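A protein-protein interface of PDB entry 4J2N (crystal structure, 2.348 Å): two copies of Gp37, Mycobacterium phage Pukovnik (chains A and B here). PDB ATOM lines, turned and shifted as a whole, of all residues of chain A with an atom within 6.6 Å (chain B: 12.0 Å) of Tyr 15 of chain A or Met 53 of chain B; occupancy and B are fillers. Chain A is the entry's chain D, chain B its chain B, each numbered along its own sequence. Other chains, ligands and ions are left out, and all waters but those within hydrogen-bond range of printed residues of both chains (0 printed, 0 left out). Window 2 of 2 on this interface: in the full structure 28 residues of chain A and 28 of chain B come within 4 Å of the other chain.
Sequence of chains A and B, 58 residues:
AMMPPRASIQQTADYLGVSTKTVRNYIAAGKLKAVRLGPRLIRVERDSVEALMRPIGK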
ATOM      1  N   MET A   3     -18.945 -36.057  -5.565  1.00  0.00           N
ATOM      2  CA  MET A   3     -18.601 -34.758  -6.141  1.00  0.00           C
ATOM      3  C   MET A   3     -17.196 -34.293  -5.762  1.00  0.00           C
ATOM      4  O   MET A   3     -16.994 -33.651  -4.727  1.00  0.00           O
ATOM      5  CB  MET A   3     -19.628 -33.706  -5.733  1.00  0.00           C
ATOM      6  CG  MET A   3     -20.637 -33.384  -6.820  1.00  0.00           C
ATOM      7  SD  MET A   3     -20.130 -31.922  -7.747  1.00  0.00           S
ATOM      8  CE  MET A   3     -19.545 -30.936  -6.362  1.00  0.00           C
ATOM      9  N   GLN A  10     -22.248 -34.370 -15.854  1.00  0.00           N
ATOM     10  CA  GLN A  10     -23.279 -35.222 -15.291  1.00  0.00           C
ATOM     11  C   GLN A  10     -23.307 -35.174 -13.768  1.00  0.00           C
ATOM     12  O   GLN A  10     -24.383 -35.073 -13.181  1.00  0.00           O
ATOM     13  CB  GLN A  10     -23.143 -36.664 -15.763  1.00  0.00           C
ATOM     14  CG  GLN A  10     -24.386 -37.499 -15.468  1.00  0.00           C
ATOM     15  CD  GLN A  10     -25.635 -36.935 -16.142  1.00  0.00           C
ATOM     16  OE1 GLN A  10     -26.590 -36.536 -15.472  1.00  0.00           O
ATOM     17  NE2 GLN A  10     -25.630 -36.898 -17.474  1.00  0.00           N
ATOM     18  N   GLN A  11     -22.142 -35.255 -13.124  1.00  0.00           N
ATOM     19  CA  GLN A  11     -22.114 -35.231 -11.658  1.00  0.00           C
ATOM     20  C   GLN A  11     -22.642 -33.911 -11.125  1.00  0.00           C
ATOM     21  O   GLN A  11     -23.284 -33.869 -10.083  1.00  0.00           O
ATOM     22  CB  GLN A  11     -20.712 -35.490 -11.105  1.00  0.00           C
ATOM     23  CG  GLN A  11     -20.299 -36.923 -11.174  1.00  0.00           C
ATOM     24  CD  GLN A  11     -18.814 -37.097 -10.945  1.00  0.00           C
ATOM     25  OE1 GLN A  11     -18.009 -36.300 -11.421  1.00  0.00           O
ATOM     26  NE2 GLN A  11     -18.444 -38.127 -10.193  1.00  0.00           N
ATOM     27  N   THR A  12     -22.357 -32.831 -11.842  1.00  0.00           N
ATOM     28  CA  THR A  12     -22.836 -31.518 -11.445  1.00  0.00           C
ATOM     29  C   THR A  12     -24.359 -31.430 -11.598  1.00  0.00           C
ATOM     30  O   THR A  12     -25.040 -30.862 -10.742  1.00  0.00           O
ATOM     31  CB  THR A  12     -22.153 -30.431 -12.278  1.00  0.00           C
ATOM     32  OG1 THR A  12     -20.741 -30.564 -12.127  1.00  0.00           O
ATOM     33  CG2 THR A  12     -22.571 -29.043 -11.828  1.00  0.00           C
ATOM     34  N   ALA A  13     -24.880 -31.997 -12.688  1.00  0.00           N
ATOM     35  CA  ALA A  13     -26.311 -32.005 -12.951  1.00  0.00           C
ATOM     36  C   ALA A  13     -27.052 -32.825 -11.896  1.00  0.00           C
ATOM     37  O   ALA A  13     -27.997 -32.335 -11.279  1.00  0.00           O
ATOM     38  CB  ALA A  13     -26.591 -32.537 -14.341  1.00  0.00           C
ATOM     39  N   ASP A  14     -26.617 -34.067 -11.690  1.00  0.00           N
ATOM     40  CA  ASP A  14     -27.137 -34.905 -10.606  1.00  0.00           C
ATOM     41  C   ASP A  14     -27.078 -34.185  -9.270  1.00  0.00           C
ATOM     42  O   ASP A  14     -28.032 -34.209  -8.492  1.00  0.00           O
ATOM     43  CB  ASP A  14     -26.354 -36.214 -10.495  1.00  0.00           C
ATOM     44  CG  ASP A  14     -26.461 -37.071 -11.745  1.00  0.00           C
ATOM     45  OD1 ASP A  14     -27.321 -36.770 -12.607  1.00  0.00           O
ATOM     46  OD2 ASP A  14     -25.688 -38.053 -11.860  1.00  0.00           O
ATOM     47  N   TYR A  15     -25.948 -33.552  -8.984  1.00  0.00           N
ATOM     48  CA  TYR A  15     -25.819 -32.897  -7.699  1.00  0.00           C
ATOM     49  C   TYR A  15     -26.857 -31.801  -7.507  1.00  0.00           C
ATOM     50  O   TYR A  15     -27.482 -31.712  -6.453  1.00  0.00           O
ATOM     51  CB  TYR A  15     -24.430 -32.323  -7.460  1.00  0.00           C
ATOM     52  CG  TYR A  15     -24.437 -31.566  -6.171  1.00  0.00           C
ATOM     53  CD1 TYR A  15     -24.184 -32.212  -4.965  1.00  0.00           C
ATOM     54  CD2 TYR A  15     -24.776 -30.225  -6.142  1.00  0.00           C
ATOM     55  CE1 TYR A  15     -24.233 -31.526  -3.765  1.00  0.00           C
ATOM     56  CE2 TYR A  15     -24.825 -29.529  -4.951  1.00  0.00           C
ATOM     57  CZ  TYR A  15     -24.560 -30.183  -3.766  1.00  0.00           C
ATOM     58  OH  TYR A  15     -24.610 -29.482  -2.589  1.00  0.00           O
ATOM     59  N   LEU A  16     -27.036 -30.960  -8.521  1.00  0.00           N
ATOM     60  CA  LEU A  16     -27.921 -29.808  -8.403  1.00  0.00           C
ATOM     61  C   LEU A  16     -29.381 -30.140  -8.731  1.00  0.00           C
ATOM     62  O   LEU A  16     -30.253 -29.292  -8.610  1.00  0.00           O
ATOM     63  CB  LEU A  16     -27.450 -28.690  -9.334  1.00  0.00           C
ATOM     64  CG  LEU A  16     -26.165 -27.918  -9.046  1.00  0.00           C
ATOM     65  CD1 LEU A  16     -25.768 -27.109 -10.285  1.00  0.00           C
ATOM     66  CD2 LEU A  16     -26.336 -27.015  -7.839  1.00  0.00           C
ATOM     67  N   GLY A  17     -29.636 -31.361  -9.182  1.00  0.00           N
ATOM     68  CA  GLY A  17     -30.961 -31.731  -9.640  1.00  0.00           C
ATOM     69  C   GLY A  17     -31.417 -30.938 -10.845  1.00  0.00           C
ATOM     70  O   GLY A  17     -32.568 -30.500 -10.910  1.00  0.00           O
ATOM     71  N   VAL A  18     -30.512 -30.741 -11.798  1.00  0.00           N
ATOM     72  CA  VAL A  18     -30.854 -30.105 -13.062  1.00  0.00           C
ATOM     73  C   VAL A  18     -30.375 -30.976 -14.208  1.00  0.00           C
ATOM     74  O   VAL A  18     -29.771 -32.034 -13.996  1.00  0.00           O
ATOM     75  CB  VAL A  18     -30.254 -28.701 -13.195  1.00  0.00           C
ATOM     76  CG1 VAL A  18     -30.817 -27.785 -12.129  1.00  0.00           C
ATOM     77  CG2 VAL A  18     -28.739 -28.759 -13.100  1.00  0.00           C
ATOM     78  N   VAL B  44     -16.161 -29.402 -14.018  1.00  0.00           N
ATOM     79  CA  VAL B  44     -16.658 -28.189 -13.384  1.00  0.00           C
ATOM     80  C   VAL B  44     -15.958 -28.016 -12.037  1.00  0.00           C
ATOM     81  O   VAL B  44     -15.658 -29.000 -11.364  1.00  0.00           O
ATOM     82  CB  VAL B  44     -18.196 -28.280 -13.170  1.00  0.00           C
ATOM     83  CG1 VAL B  44     -18.719 -27.055 -12.441  1.00  0.00           C
ATOM     84  CG2 VAL B  44     -18.925 -28.470 -14.505  1.00  0.00           C
ATOM     85  N   GLU B  45     -15.683 -26.780 -11.640  1.00  0.00           N
ATOM     86  CA  GLU B  45     -15.024 -26.536 -10.359  1.00  0.00           C
ATOM     87  C   GLU B  45     -16.020 -26.523  -9.188  1.00  0.00           C
ATOM     88  O   GLU B  45     -16.924 -25.684  -9.122  1.00  0.00           O
ATOM     89  CB  GLU B  45     -14.218 -25.238 -10.410  1.00  0.00           C
ATOM     90  CG  GLU B  45     -13.180 -25.205 -11.537  1.00  0.00           C
ATOM     91  CD  GLU B  45     -12.422 -23.878 -11.609  1.00  0.00           C
ATOM     92  OE1 GLU B  45     -12.840 -22.916 -10.925  1.00  0.00           O
ATOM     93  OE2 GLU B  45     -11.407 -23.794 -12.345  1.00  0.00           O
ATOM     94  N   ARG B  46     -15.835 -27.454  -8.257  1.00  0.00           N
ATOM     95  CA  ARG B  46     -16.734 -27.595  -7.121  1.00  0.00           C
ATOM     96  C   ARG B  46     -17.030 -26.265  -6.444  1.00  0.00           C
ATOM     97  O   ARG B  46     -18.174 -25.952  -6.124  1.00  0.00           O
ATOM     98  CB  ARG B  46     -16.156 -28.575  -6.109  1.00  0.00           C
ATOM     99  CG  ARG B  46     -17.104 -28.871  -4.971  1.00  0.00           C
ATOM    100  CD  ARG B  46     -16.638 -30.072  -4.206  1.00  0.00           C
ATOM    101  NE  ARG B  46     -15.387 -29.817  -3.502  1.00  0.00           N
ATOM    102  CZ  ARG B  46     -14.563 -30.780  -3.104  1.00  0.00           C
ATOM    103  NH1 ARG B  46     -14.862 -32.051  -3.356  1.00  0.00           N
ATOM    104  NH2 ARG B  46     -13.440 -30.479  -2.465  1.00  0.00           N
ATOM    105  N   ASP B  47     -15.993 -25.475  -6.234  1.00  0.00           N
ATOM    106  CA  ASP B  47     -16.166 -24.176  -5.613  1.00  0.00           C
ATOM    107  C   ASP B  47     -17.269 -23.353  -6.256  1.00  0.00           C
ATOM    108  O   ASP B  47     -18.111 -22.797  -5.556  1.00  0.00           O
ATOM    109  CB  ASP B  47     -14.848 -23.422  -5.660  1.00  0.00           C
ATOM    110  CG  ASP B  47     -13.692 -24.297  -5.255  1.00  0.00           C
ATOM    111  OD1 ASP B  47     -13.560 -24.556  -4.033  1.00  0.00           O
ATOM    112  OD2 ASP B  47     -12.946 -24.754  -6.156  1.00  0.00           O
ATOM    113  N   SER B  48     -17.271 -23.264  -7.583  1.00  0.00           N
ATOM    114  CA  SER B  48     -18.270 -22.435  -8.251  1.00  0.00           C
ATOM    115  C   SER B  48     -19.676 -23.025  -8.131  1.00  0.00           C
ATOM    116  O   SER B  48     -20.664 -22.298  -8.106  1.00  0.00           O
ATOM    117  CB  SER B  48     -17.921 -22.203  -9.718  1.00  0.00           C
ATOM    118  OG  SER B  48     -18.031 -23.398 -10.465  1.00  0.00           O
ATOM    119  N   VAL B  49     -19.753 -24.347  -8.073  1.00  0.00           N
ATOM    120  CA  VAL B  49     -21.021 -25.018  -7.864  1.00  0.00           C
ATOM    121  C   VAL B  49     -21.564 -24.648  -6.494  1.00  0.00           C
ATOM    122  O   VAL B  49     -22.758 -24.425  -6.329  1.00  0.00           O
ATOM    123  CB  VAL B  49     -20.861 -26.541  -7.913  1.00  0.00           C
ATOM    124  CG1 VAL B  49     -22.224 -27.207  -7.825  1.00  0.00           C
ATOM    125  CG2 VAL B  49     -20.152 -26.957  -9.195  1.00  0.00           C
ATOM    126  N   GLU B  50     -20.662 -24.588  -5.518  1.00  0.00           N
ATOM    127  CA  GLU B  50     -21.019 -24.294  -4.138  1.00  0.00           C
ATOM    128  C   GLU B  50     -21.541 -22.870  -4.011  1.00  0.00           C
ATOM    129  O   GLU B  50     -22.544 -22.620  -3.331  1.00  0.00           O
ATOM    130  CB  GLU B  50     -19.811 -24.501  -3.221  1.00  0.00           C
ATOM    131  CG  GLU B  50     -20.069 -25.416  -2.038  1.00  0.00           C
ATOM    132  CD  GLU B  50     -20.132 -26.897  -2.413  1.00  0.00           C
ATOM    133  OE1 GLU B  50     -19.150 -27.629  -2.134  1.00  0.00           O
ATOM    134  OE2 GLU B  50     -21.171 -27.336  -2.955  1.00  0.00           O
ATOM    135  N   ALA B  51     -20.863 -21.942  -4.676  1.00  0.00           N
ATOM    136  CA  ALA B  51     -21.247 -20.534  -4.638  1.00  0.00           C
ATOM    137  C   ALA B  51     -22.458 -20.204  -5.523  1.00  0.00           C
ATOM    138  O   ALA B  51     -23.042 -19.121  -5.406  1.00  0.00           O
ATOM    139  CB  ALA B  51     -20.064 -19.663  -5.020  1.00  0.00           C
ATOM    140  N   LEU B  52     -22.831 -21.119  -6.415  1.00  0.00           N
ATOM    141  CA  LEU B  52     -24.030 -20.916  -7.231  1.00  0.00           C
ATOM    142  C   LEU B  52     -25.305 -21.045  -6.390  1.00  0.00           C
ATOM    143  O   LEU B  52     -26.306 -20.377  -6.655  1.00  0.00           O
ATOM    144  CB  LEU B  52     -24.082 -21.916  -8.385  1.00  0.00           C
ATOM    145  CG  LEU B  52     -25.378 -21.904  -9.192  1.00  0.00           C
ATOM    146  CD1 LEU B  52     -25.371 -20.757 -10.179  1.00  0.00           C
ATOM    147  CD2 LEU B  52     -25.578 -23.224  -9.913  1.00  0.00           C
ATOM    148  N   MET B  53     -25.261 -21.917  -5.388  1.00  0.00           N
ATOM    149  CA  MET B  53     -26.416 -22.159  -4.539  1.00  0.00           C
ATOM    150  C   MET B  53     -26.536 -21.114  -3.436  1.00  0.00           C
ATOM    151  O   MET B  53     -25.930 -21.251  -2.379  1.00  0.00           O
ATOM    152  CB  MET B  53     -26.355 -23.574  -3.948  1.00  0.00           C
ATOM    153  CG  MET B  53     -26.340 -24.652  -5.020  1.00  0.00           C
ATOM    154  SD  MET B  53     -26.284 -26.328  -4.367  1.00  0.00           S
ATOM    155  CE  MET B  53     -24.885 -26.202  -3.266  1.00  0.00           C
ATOM    156  N   ARG B  54     -27.327 -20.076  -3.700  1.00  0.00           N
ATOM    157  CA  ARG B  54     -27.612 -19.008  -2.732  1.00  0.00           C
ATOM    158  C   ARG B  54     -28.750 -19.376  -1.775  1.00  0.00           C
ATOM    159  O   ARG B  54     -29.892 -19.551  -2.208  1.00  0.00           O
ATOM    160  CB  ARG B  54     -27.997 -17.721  -3.476  1.00  0.00           C
ATOM    161  CG  ARG B  54     -26.838 -16.977  -4.138  1.00  0.00           C
ATOM    162  CD  ARG B  54     -27.308 -15.973  -5.220  1.00  0.00           C
ATOM    163  NE  ARG B  54     -28.629 -15.371  -4.983  1.00  0.00           N
ATOM    164  CZ  ARG B  54     -28.847 -14.227  -4.330  1.00  0.00           C
ATOM    165  NH1 ARG B  54     -27.833 -13.542  -3.813  1.00  0.00           N
ATOM    166  NH2 ARG B  54     -30.088 -13.770  -4.186  1.00  0.00           N
ATOM    167  N   PRO B  55     -28.450 -19.487  -0.467  1.00  0.00           N
ATOM    168  CA  PRO B  55     -29.503 -19.753   0.524  1.00  0.00           C
ATOM    169  C   PRO B  55     -30.616 -18.701   0.496  1.00  0.00           C
ATOM    170  O   PRO B  55     -30.434 -17.619  -0.067  1.00  0.00           O
ATOM    171  CB  PRO B  55     -28.752 -19.700   1.859  1.00  0.00           C
ATOM    172  CG  PRO B  55     -27.352 -20.085   1.520  1.00  0.00           C
ATOM    173  CD  PRO B  55     -27.100 -19.546   0.129  1.00  0.00           C
ATOM    174  N   ILE B  56     -31.760 -19.031   1.092  1.00  0.00           N
ATOM    175  CA  ILE B  56     -32.890 -18.110   1.171  1.00  0.00           C
ATOM    176  C   ILE B  56     -33.255 -17.793   2.621  1.00  0.00           C
ATOM    177  O   ILE B  56     -33.452 -16.631   2.983  1.00  0.00           O
ATOM    178  CB  ILE B  56     -34.125 -18.673   0.444  1.00  0.00           C
ATOM    179  CG1 ILE B  56     -33.818 -18.877  -1.039  1.00  0.00           C
ATOM    180  CG2 ILE B  56     -35.319 -17.740   0.620  1.00  0.00           C
ATOM    181  CD1 ILE B  56     -34.821 -19.737  -1.742  1.00  0.00           C
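Among the printed residues, pairs that only touch across the chains: Thr 12 of chain A with Val 44 of chain B (3.6 Å), Tyr 15 of chain A with Met 53 of chain B (3.4 Å), Leu 16 of chain A with Leu 52 of chain B (3.9 Å) and Leu 16 of chain A with Met 53 of chain B (3.5 Å).
Thr 12 of chain A touches one residue of chain B. Of chain B, only Met 53 comes within 4 Å of Tyr 15 of chain A. Of chain B, only Leu 52 (3.9 Å) and Met 53 (3.5 Å) come within 4 Å of Leu 16 of chain A. No residue of chain B comes within 4 Å of Gly 17 of chain A. No residue of chain B comes within 4 Å of Val 18 of chain A. Of the printed residues of chain A, Val 44 of chain B touches Thr 12. Printed residues of chain A within 4 Å of Arg 46 of chain B: Met 3. Asp 47 of chain B touches none of the printed residues of chain A. Of the printed residues of chain A, Leu 52 of chain B touches Leu 16.
NH1 of Arg 46 of chain B is in hydrogen-bond range of O of Met 3 of chain A, at 3.0 Å.
Hydrophobic or aromatic side chains of chain A that line the printed part of chain B: Met 3, Tyr 15 and Leu 16.
No position is printed for both chains. Of the 5 pairs that touch across the chains among the printed residues, none has its exchanged pair printed and touching as well.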
